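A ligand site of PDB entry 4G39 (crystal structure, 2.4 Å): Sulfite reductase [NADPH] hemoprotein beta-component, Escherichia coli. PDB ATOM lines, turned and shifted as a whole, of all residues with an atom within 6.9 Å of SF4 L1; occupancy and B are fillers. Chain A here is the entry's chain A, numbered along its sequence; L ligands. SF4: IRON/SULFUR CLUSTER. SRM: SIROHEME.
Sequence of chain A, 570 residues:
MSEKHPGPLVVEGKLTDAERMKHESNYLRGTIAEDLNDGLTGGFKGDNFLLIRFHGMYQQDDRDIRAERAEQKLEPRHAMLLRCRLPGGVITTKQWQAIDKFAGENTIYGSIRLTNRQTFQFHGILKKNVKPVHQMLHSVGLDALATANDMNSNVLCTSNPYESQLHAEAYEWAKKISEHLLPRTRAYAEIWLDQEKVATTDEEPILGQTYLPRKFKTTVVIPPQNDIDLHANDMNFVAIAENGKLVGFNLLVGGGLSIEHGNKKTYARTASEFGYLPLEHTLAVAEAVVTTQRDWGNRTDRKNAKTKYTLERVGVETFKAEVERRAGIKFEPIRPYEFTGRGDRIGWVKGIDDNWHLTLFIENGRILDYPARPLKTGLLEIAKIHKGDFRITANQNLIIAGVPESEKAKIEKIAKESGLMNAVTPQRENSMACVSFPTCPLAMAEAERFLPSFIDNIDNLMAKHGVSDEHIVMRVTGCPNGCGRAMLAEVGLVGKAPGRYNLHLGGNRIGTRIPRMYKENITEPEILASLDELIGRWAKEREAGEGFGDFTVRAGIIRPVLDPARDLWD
The side-chain hydroxyl of Thr 477 is in hydrogen-bond range of the backbone NH of Cys 483 (3.3 Å).
The side-chain sulfur (SG) of Cys 434 lies close to the backbone NH (N) of Gly 478 (3.1 Å).
N of Cys 434 lies within hydrogen-bond range of O of Val 476 (3.2 Å).
The side-chain sulfur of Cys 479 lies close to the backbone NH of Asn 481 (3.5 Å).
The side-chain hydroxyl (OG1) of Thr 477 is in hydrogen-bond range of the backbone NH (N) of Gly 484.
O of Gly 478 sits at hydrogen-bond distance from N of Met 444, 3.1 Å away.
O of Gly 478 is in hydrogen-bond range of N of Ala 445.
O of Ala 445 is in hydrogen-bond range of OG of Ser 436 (2.7 Å).
Merely in contact with SF4 L1: Ala 443 (3.7 Å), Gly 478 (3.5 Å) and Gly 482 (3.996 Å).
Hydrophobic or aromatic side chains within 4 Å of SF4 L1: Ala 443.
Ten residues have an atom within 4 Å of SF4 L1: Cys 434, Ser 436, Cys 440, Ala 443, Thr 477, Gly 478, Cys 479, Asn 481, Gly 482 and Cys 483.
The backbone NH (N) of Cys 483 sits close to a sulfur (S2) of SF4 L1, 3.6 Å away.
FE4 of SF4 L1 is bound by SG of Cys 483 (2.1 Å).
The side-chain sulfur (SG) of Cys 434 binds an iron atom (FE1) of SF4 L1 (2.2 Å).
N of Cys 479 lies close to S4 of SF4 L1 (3.7 Å).
The side-chain sulfur of Cys 479 binds an iron atom (FE3) of SF4 L1 (2.2 Å).
An iron atom (FE2) of SF4 L1 is bound by the side-chain sulfur of Cys 440 (2.2 Å).
A sulfur (S2) of SF4 L1 sits close to the side-chain hydroxyl of Thr 477 (3.4 Å).
The side-chain amide nitrogen (ND2) of Asn 481 sits close to a sulfur (S1) of SF4 L1, 3.6 Å away.
The backbone NH (N) of Ser 436 sits close to a sulfur (S3) of SF4 L1, at 3.7 Å.
An iron atom (FE) of SRM L2 is bound by the side-chain sulfur (SG) of Cys 483 (2.4 Å).
The backbone NH (N) of Cys 440 sits at hydrogen-bond distance from an oxygen (O1A) of SRM L2 (3.4 Å).
The backbone NH (N) of Val 435 lies within hydrogen-bond range of an oxygen (O3B) of SRM L2, at 3.4 Å.
An oxygen (O1A) of SRM L2 lies within hydrogen-bond range of the side-chain hydroxyl (OG1) of Thr 439 (3.0 Å).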
ATOM      1  N   ALA A 433     -16.708  27.550 -18.238  1.00  0.00           N
ATOM      2  CA  ALA A 433     -15.623  27.174 -17.347  1.00  0.00           C
ATOM      3  C   ALA A 433     -14.783  28.412 -17.030  1.00  0.00           C
ATOM      4  O   ALA A 433     -14.660  29.329 -17.864  1.00  0.00           O
ATOM      5  CB  ALA A 433     -14.763  26.123 -17.994  1.00  0.00           C
ATOM      6  N   CYS A 434     -14.223  28.430 -15.819  1.00  0.00           N
ATOM      7  CA  CYS A 434     -13.254  29.446 -15.421  1.00  0.00           C
ATOM      8  C   CYS A 434     -11.897  29.190 -16.097  1.00  0.00           C
ATOM      9  O   CYS A 434     -11.708  28.188 -16.814  1.00  0.00           O
ATOM     10  CB  CYS A 434     -13.070  29.415 -13.920  1.00  0.00           C
ATOM     11  SG  CYS A 434     -12.165  27.972 -13.453  1.00  0.00           S
ATOM     12  N   VAL A 435     -10.952  30.105 -15.858  1.00  0.00           N
ATOM     13  CA  VAL A 435      -9.623  30.052 -16.457  1.00  0.00           C
ATOM     14  C   VAL A 435      -8.774  28.871 -15.947  1.00  0.00           C
ATOM     15  O   VAL A 435      -8.271  28.076 -16.738  1.00  0.00           O
ATOM     16  CB  VAL A 435      -8.879  31.410 -16.303  1.00  0.00           C
ATOM     17  CG1 VAL A 435      -7.410  31.272 -16.614  1.00  0.00           C
ATOM     18  CG2 VAL A 435      -9.498  32.435 -17.227  1.00  0.00           C
ATOM     19  N   SER A 436      -8.630  28.743 -14.632  1.00  0.00           N
ATOM     20  CA  SER A 436      -7.840  27.645 -14.082  1.00  0.00           C
ATOM     21  C   SER A 436      -6.403  27.589 -14.643  1.00  0.00           C
ATOM     22  O   SER A 436      -5.819  28.637 -14.957  1.00  0.00           O
ATOM     23  CB  SER A 436      -8.533  26.304 -14.344  1.00  0.00           C
ATOM     24  OG  SER A 436      -7.997  25.328 -13.494  1.00  0.00           O
ATOM     25  N   PHE A 437      -5.840  26.388 -14.747  1.00  0.00           N
ATOM     26  CA  PHE A 437      -4.507  26.187 -15.354  1.00  0.00           C
ATOM     27  C   PHE A 437      -4.521  26.672 -16.814  1.00  0.00           C
ATOM     28  O   PHE A 437      -5.539  26.560 -17.510  1.00  0.00           O
ATOM     29  CB  PHE A 437      -4.075  24.708 -15.306  1.00  0.00           C
ATOM     30  CG  PHE A 437      -4.051  24.102 -13.914  1.00  0.00           C
ATOM     31  CD1 PHE A 437      -3.108  24.492 -12.976  1.00  0.00           C
ATOM     32  CD2 PHE A 437      -4.967  23.118 -13.567  1.00  0.00           C
ATOM     33  CE1 PHE A 437      -3.079  23.915 -11.716  1.00  0.00           C
ATOM     34  CE2 PHE A 437      -4.951  22.537 -12.310  1.00  0.00           C
ATOM     35  CZ  PHE A 437      -4.010  22.925 -11.385  1.00  0.00           C
ATOM     36  N   THR A 439      -2.561  29.518 -15.924  1.00  0.00           N
ATOM     37  CA  THR A 439      -2.251  30.808 -15.318  1.00  0.00           C
ATOM     38  C   THR A 439      -2.761  31.052 -13.881  1.00  0.00           C
ATOM     39  O   THR A 439      -2.170  31.848 -13.130  1.00  0.00           O
ATOM     40  CB  THR A 439      -2.717  31.974 -16.218  1.00  0.00           C
ATOM     41  OG1 THR A 439      -4.120  31.838 -16.494  1.00  0.00           O
ATOM     42  CG2 THR A 439      -1.938  31.957 -17.532  1.00  0.00           C
ATOM     43  N   CYS A 440      -3.834  30.384 -13.479  1.00  0.00           N
ATOM     44  CA  CYS A 440      -4.357  30.618 -12.140  1.00  0.00           C
ATOM     45  C   CYS A 440      -3.564  29.911 -11.040  1.00  0.00           C
ATOM     46  O   CYS A 440      -3.492  28.695 -11.004  1.00  0.00           O
ATOM     47  CB  CYS A 440      -5.821  30.207 -12.029  1.00  0.00           C
ATOM     48  SG  CYS A 440      -6.516  30.768 -10.444  1.00  0.00           S
ATOM     49  N   PRO A 441      -2.989  30.696 -10.122  1.00  0.00           N
ATOM     50  CA  PRO A 441      -2.167  30.124  -9.053  1.00  0.00           C
ATOM     51  C   PRO A 441      -2.997  29.295  -8.062  1.00  0.00           C
ATOM     52  O   PRO A 441      -2.440  28.526  -7.277  1.00  0.00           O
ATOM     53  CB  PRO A 441      -1.592  31.357  -8.344  1.00  0.00           C
ATOM     54  CG  PRO A 441      -2.594  32.473  -8.656  1.00  0.00           C
ATOM     55  CD  PRO A 441      -3.080  32.170 -10.048  1.00  0.00           C
ATOM     56  N   LEU A 442      -4.309  29.436  -8.122  1.00  0.00           N
ATOM     57  CA  LEU A 442      -5.181  28.819  -7.125  1.00  0.00           C
ATOM     58  C   LEU A 442      -5.859  27.555  -7.661  1.00  0.00           C
ATOM     59  O   LEU A 442      -6.610  26.876  -6.964  1.00  0.00           O
ATOM     60  CB  LEU A 442      -6.236  29.836  -6.623  1.00  0.00           C
ATOM     61  CG  LEU A 442      -5.741  31.217  -6.145  1.00  0.00           C
ATOM     62  CD1 LEU A 442      -6.881  32.123  -5.664  1.00  0.00           C
ATOM     63  CD2 LEU A 442      -4.708  31.057  -5.035  1.00  0.00           C
ATOM     64  N   ALA A 443      -5.591  27.226  -8.924  1.00  0.00           N
ATOM     65  CA  ALA A 443      -6.310  26.137  -9.565  1.00  0.00           C
ATOM     66  C   ALA A 443      -6.079  24.753  -8.914  1.00  0.00           C
ATOM     67  O   ALA A 443      -4.948  24.407  -8.522  1.00  0.00           O
ATOM     68  CB  ALA A 443      -6.013  26.109 -11.058  1.00  0.00           C
ATOM     69  N   MET A 444      -7.153  23.957  -8.818  1.00  0.00           N
ATOM     70  CA  MET A 444      -7.053  22.569  -8.352  1.00  0.00           C
ATOM     71  C   MET A 444      -7.198  21.559  -9.484  1.00  0.00           C
ATOM     72  O   MET A 444      -6.438  20.602  -9.578  1.00  0.00           O
ATOM     73  CB  MET A 444      -8.064  22.299  -7.245  1.00  0.00           C
ATOM     74  CG  MET A 444      -7.872  23.223  -6.034  1.00  0.00           C
ATOM     75  SD  MET A 444      -9.113  23.091  -4.722  1.00  0.00           S
ATOM     76  CE  MET A 444      -8.624  21.585  -3.866  1.00  0.00           C
ATOM     77  N   ALA A 445      -8.197  21.778 -10.342  1.00  0.00           N
ATOM     78  CA  ALA A 445      -8.442  20.918 -11.481  1.00  0.00           C
ATOM     79  C   ALA A 445      -8.617  21.783 -12.744  1.00  0.00           C
ATOM     80  O   ALA A 445      -9.015  22.934 -12.657  1.00  0.00           O
ATOM     81  CB  ALA A 445      -9.687  20.071 -11.224  1.00  0.00           C
ATOM     82  N   ALA A 447     -10.205  23.540 -15.924  1.00  0.00           N
ATOM     83  CA  ALA A 447     -11.555  23.956 -16.248  1.00  0.00           C
ATOM     84  C   ALA A 447     -11.695  24.415 -17.720  1.00  0.00           C
ATOM     85  O   ALA A 447     -12.329  23.742 -18.508  1.00  0.00           O
ATOM     86  CB  ALA A 447     -12.033  25.025 -15.279  1.00  0.00           C
ATOM     87  N   VAL A 476     -18.028  24.317 -15.195  1.00  0.00           N
ATOM     88  CA  VAL A 476     -16.883  23.753 -14.501  1.00  0.00           C
ATOM     89  C   VAL A 476     -16.048  24.858 -13.902  1.00  0.00           C
ATOM     90  O   VAL A 476     -15.687  25.817 -14.587  1.00  0.00           O
ATOM     91  CB  VAL A 476     -15.991  22.982 -15.471  1.00  0.00           C
ATOM     92  CG1 VAL A 476     -14.857  22.259 -14.701  1.00  0.00           C
ATOM     93  CG2 VAL A 476     -16.818  21.998 -16.271  1.00  0.00           C
ATOM     94  N   THR A 477     -15.753  24.734 -12.626  1.00  0.00           N
ATOM     95  CA  THR A 477     -14.914  25.697 -11.942  1.00  0.00           C
ATOM     96  C   THR A 477     -13.686  24.952 -11.407  1.00  0.00           C
ATOM     97  O   THR A 477     -13.794  23.815 -10.924  1.00  0.00           O
ATOM     98  CB  THR A 477     -15.738  26.467 -10.861  1.00  0.00           C
ATOM     99  OG1 THR A 477     -15.173  27.761 -10.638  1.00  0.00           O
ATOM    100  CG2 THR A 477     -15.823  25.700  -9.535  1.00  0.00           C
ATOM    101  N   GLY A 478     -12.513  25.565 -11.526  1.00  0.00           N
ATOM    102  CA  GLY A 478     -11.243  24.915 -11.193  1.00  0.00           C
ATOM    103  C   GLY A 478     -10.967  24.679  -9.717  1.00  0.00           C
ATOM    104  O   GLY A 478     -10.185  23.796  -9.352  1.00  0.00           O
ATOM    105  N   CYS A 479     -11.612  25.470  -8.867  1.00  0.00           N
ATOM    106  CA  CYS A 479     -11.531  25.319  -7.418  1.00  0.00           C
ATOM    107  C   CYS A 479     -12.793  25.950  -6.794  1.00  0.00           C
ATOM    108  O   CYS A 479     -13.599  26.527  -7.508  1.00  0.00           O
ATOM    109  CB  CYS A 479     -10.252  25.971  -6.875  1.00  0.00           C
ATOM    110  SG  CYS A 479     -10.382  27.765  -6.626  1.00  0.00           S
ATOM    111  N   PRO A 480     -12.985  25.790  -5.471  1.00  0.00           N
ATOM    112  CA  PRO A 480     -14.238  26.233  -4.851  1.00  0.00           C
ATOM    113  C   PRO A 480     -14.453  27.756  -4.790  1.00  0.00           C
ATOM    114  O   PRO A 480     -15.514  28.184  -4.324  1.00  0.00           O
ATOM    115  CB  PRO A 480     -14.161  25.649  -3.430  1.00  0.00           C
ATOM    116  CG  PRO A 480     -12.691  25.511  -3.168  1.00  0.00           C
ATOM    117  CD  PRO A 480     -12.099  25.111  -4.505  1.00  0.00           C
ATOM    118  N   ASN A 481     -13.493  28.549  -5.258  1.00  0.00           N
ATOM    119  CA  ASN A 481     -13.724  30.003  -5.321  1.00  0.00           C
ATOM    120  C   ASN A 481     -14.931  30.334  -6.193  1.00  0.00           C
ATOM    121  O   ASN A 481     -15.606  31.346  -5.980  1.00  0.00           O
ATOM    122  CB  ASN A 481     -12.481  30.748  -5.808  1.00  0.00           C
ATOM    123  CG  ASN A 481     -11.423  30.836  -4.749  1.00  0.00           C
ATOM    124  OD1 ASN A 481     -11.722  30.768  -3.546  1.00  0.00           O
ATOM    125  ND2 ASN A 481     -10.175  30.998  -5.158  1.00  0.00           N
ATOM    126  N   GLY A 482     -15.168  29.487  -7.197  1.00  0.00           N
ATOM    127  CA  GLY A 482     -16.424  29.475  -7.930  1.00  0.00           C
ATOM    128  C   GLY A 482     -16.520  30.379  -9.135  1.00  0.00           C
ATOM    129  O   GLY A 482     -17.624  30.585  -9.653  1.00  0.00           O
ATOM    130  N   CYS A 483     -15.389  30.894  -9.593  1.00  0.00           N
ATOM    131  CA  CYS A 483     -15.378  31.838 -10.710  1.00  0.00           C
ATOM    132  C   CYS A 483     -16.186  31.377 -11.905  1.00  0.00           C
ATOM    133  O   CYS A 483     -16.762  32.197 -12.615  1.00  0.00           O
ATOM    134  CB  CYS A 483     -13.962  32.131 -11.163  1.00  0.00           C
ATOM    135  SG  CYS A 483     -12.893  32.607  -9.812  1.00  0.00           S
ATOM    136  N   GLY A 484     -16.233  30.074 -12.122  1.00  0.00           N
ATOM    137  CA  GLY A 484     -17.017  29.520 -13.231  1.00  0.00           C
ATOM    138  C   GLY A 484     -18.517  29.459 -12.966  1.00  0.00           C
ATOM    139  O   GLY A 484     -19.285  29.060 -13.850  1.00  0.00           O
HETATM  140 FE1  SF4 L   1     -11.080  28.728 -11.695  1.00  0.00          FE
HETATM  141 FE2  SF4 L   1      -8.593  29.980 -10.542  1.00  0.00          FE
HETATM  142 FE3  SF4 L   1     -10.494  28.621  -8.655  1.00  0.00          FE
HETATM  143 FE4  SF4 L   1     -11.334  31.175 -10.126  1.00  0.00          FE
HETATM  144  S1  SF4 L   1      -9.697  30.678  -8.761  1.00  0.00           S
HETATM  145  S2  SF4 L   1     -12.218  29.168  -9.873  1.00  0.00           S
HETATM  146  S3  SF4 L   1     -10.149  30.676 -11.903  1.00  0.00           S
HETATM  147  S4  SF4 L   1      -9.425  27.963 -10.474  1.00  0.00           S
HETATM  148 FE   SRM L   2     -12.645  35.008  -9.950  1.00  0.00          FE
HETATM  149  CHA SRM L   2      -9.946  34.878  -7.879  1.00  0.00           C
HETATM  150  CHB SRM L   2     -10.708  34.481 -12.601  1.00  0.00           C
HETATM  151  CHC SRM L   2     -15.274  35.692 -11.949  1.00  0.00           C
HETATM  152  CHD SRM L   2     -14.703  34.414  -7.367  1.00  0.00           C
HETATM  153  NA  SRM L   2     -10.709  34.765 -10.196  1.00  0.00           N
HETATM  154  C1A SRM L   2      -9.738  34.817  -9.245  1.00  0.00           C
HETATM  155  C2A SRM L   2      -8.383  34.984  -9.860  1.00  0.00           C
HETATM  156  CMA SRM L   2      -8.087  36.479  -9.979  1.00  0.00           C
HETATM  157  CDA SRM L   2      -7.296  34.158  -9.150  1.00  0.00           C
HETATM  158  CEA SRM L   2      -6.456  34.883  -8.099  1.00  0.00           C
HETATM  159  O3A SRM L   2      -6.953  35.458  -7.107  1.00  0.00           O
HETATM  160  O4A SRM L   2      -5.215  34.895  -8.200  1.00  0.00           O
HETATM  161  C3A SRM L   2      -8.639  34.381 -11.177  1.00  0.00           C
HETATM  162  CAA SRM L   2      -7.532  34.662 -12.152  1.00  0.00           C
HETATM  163  CBA SRM L   2      -7.240  33.366 -12.901  1.00  0.00           C
HETATM  164  CCA SRM L   2      -6.455  33.690 -14.156  1.00  0.00           C
HETATM  165  O1A SRM L   2      -5.237  33.438 -14.247  1.00  0.00           O
HETATM  166  O2A SRM L   2      -6.998  34.225 -15.142  1.00  0.00           O
HETATM  167  C4A SRM L   2     -10.095  34.508 -11.366  1.00  0.00           C
HETATM  168  NB  SRM L   2     -12.907  35.147 -11.874  1.00  0.00           N
HETATM  169  C1B SRM L   2     -12.019  34.823 -12.831  1.00  0.00           C
HETATM  170  C2B SRM L   2     -12.688  34.906 -14.170  1.00  0.00           C
HETATM  171  CMB SRM L   2     -11.720  35.341 -15.262  1.00  0.00           C
HETATM  172  CDB SRM L   2     -13.315  33.564 -14.518  1.00  0.00           C
HETATM  173  CEB SRM L   2     -13.589  33.500 -15.998  1.00  0.00           C
HETATM  174  O3B SRM L   2     -13.176  32.533 -16.694  1.00  0.00           O
HETATM  175  O4B SRM L   2     -14.224  34.416 -16.553  1.00  0.00           O
HETATM  176  C3B SRM L   2     -13.698  35.974 -13.877  1.00  0.00           C
HETATM  177  CAB SRM L   2     -13.149  37.355 -14.122  1.00  0.00           C
HETATM  178  CBB SRM L   2     -14.159  38.354 -13.537  1.00  0.00           C
HETATM  179  CCB SRM L   2     -13.869  39.782 -13.943  1.00  0.00           C
HETATM  180  O1B SRM L   2     -13.834  40.123 -15.151  1.00  0.00           O
HETATM  181  O2B SRM L   2     -13.671  40.661 -13.084  1.00  0.00           O
HETATM  182  C4B SRM L   2     -14.026  35.586 -12.498  1.00  0.00           C
HETATM  183  NC  SRM L   2     -14.603  35.004  -9.720  1.00  0.00           N
HETATM  184  C1C SRM L   2     -15.536  35.303 -10.656  1.00  0.00           C
HETATM  185  C2C SRM L   2     -16.924  35.172 -10.159  1.00  0.00           C
HETATM  186  CDC SRM L   2     -18.135  34.998 -11.046  1.00  0.00           C
HETATM  187  CEC SRM L   2     -18.830  36.321 -11.254  1.00  0.00           C
HETATM  188  O3C SRM L   2     -18.421  37.348 -10.678  1.00  0.00           O
HETATM  189  O4C SRM L   2     -19.809  36.409 -12.039  1.00  0.00           O
HETATM  190  C3C SRM L   2     -16.743  34.535  -8.859  1.00  0.00           C
HETATM  191  CAC SRM L   2     -17.793  33.772  -8.078  1.00  0.00           C
HETATM  192  CBC SRM L   2     -18.819  34.739  -7.506  1.00  0.00           C
HETATM  193  CCC SRM L   2     -18.300  35.254  -6.175  1.00  0.00           C
HETATM  194  O1C SRM L   2     -17.666  36.337  -6.124  1.00  0.00           O
HETATM  195  O2C SRM L   2     -18.496  34.608  -5.120  1.00  0.00           O
HETATM  196  C4C SRM L   2     -15.280  34.657  -8.607  1.00  0.00           C
HETATM  197  ND  SRM L   2     -12.379  34.757  -8.006  1.00  0.00           N
HETATM  198  C1D SRM L   2     -13.356  34.513  -7.094  1.00  0.00           C
HETATM  199  C2D SRM L   2     -12.815  34.272  -5.737  1.00  0.00           C
HETATM  200  CAD SRM L   2     -13.584  33.935  -4.490  1.00  0.00           C
HETATM  201  CBD SRM L   2     -13.957  35.248  -3.830  1.00  0.00           C
HETATM  202  CCD SRM L   2     -14.615  34.945  -2.503  1.00  0.00           C
HETATM  203  O1D SRM L   2     -15.648  35.546  -2.155  1.00  0.00           O
HETATM  204  O2D SRM L   2     -14.142  34.058  -1.759  1.00  0.00           O
HETATM  205  C3D SRM L   2     -11.363  34.424  -5.877  1.00  0.00           C
HETATM  206  CDD SRM L   2     -10.287  34.278  -4.822  1.00  0.00           C
HETATM  207  CED SRM L   2     -10.300  35.405  -3.805  1.00  0.00           C
HETATM  208  O3D SRM L   2     -10.162  36.603  -4.122  1.00  0.00           O
HETATM  209  O4D SRM L   2     -10.457  35.148  -2.580  1.00  0.00           O
HETATM  210  C4D SRM L   2     -11.200  34.719  -7.322  1.00  0.00           C
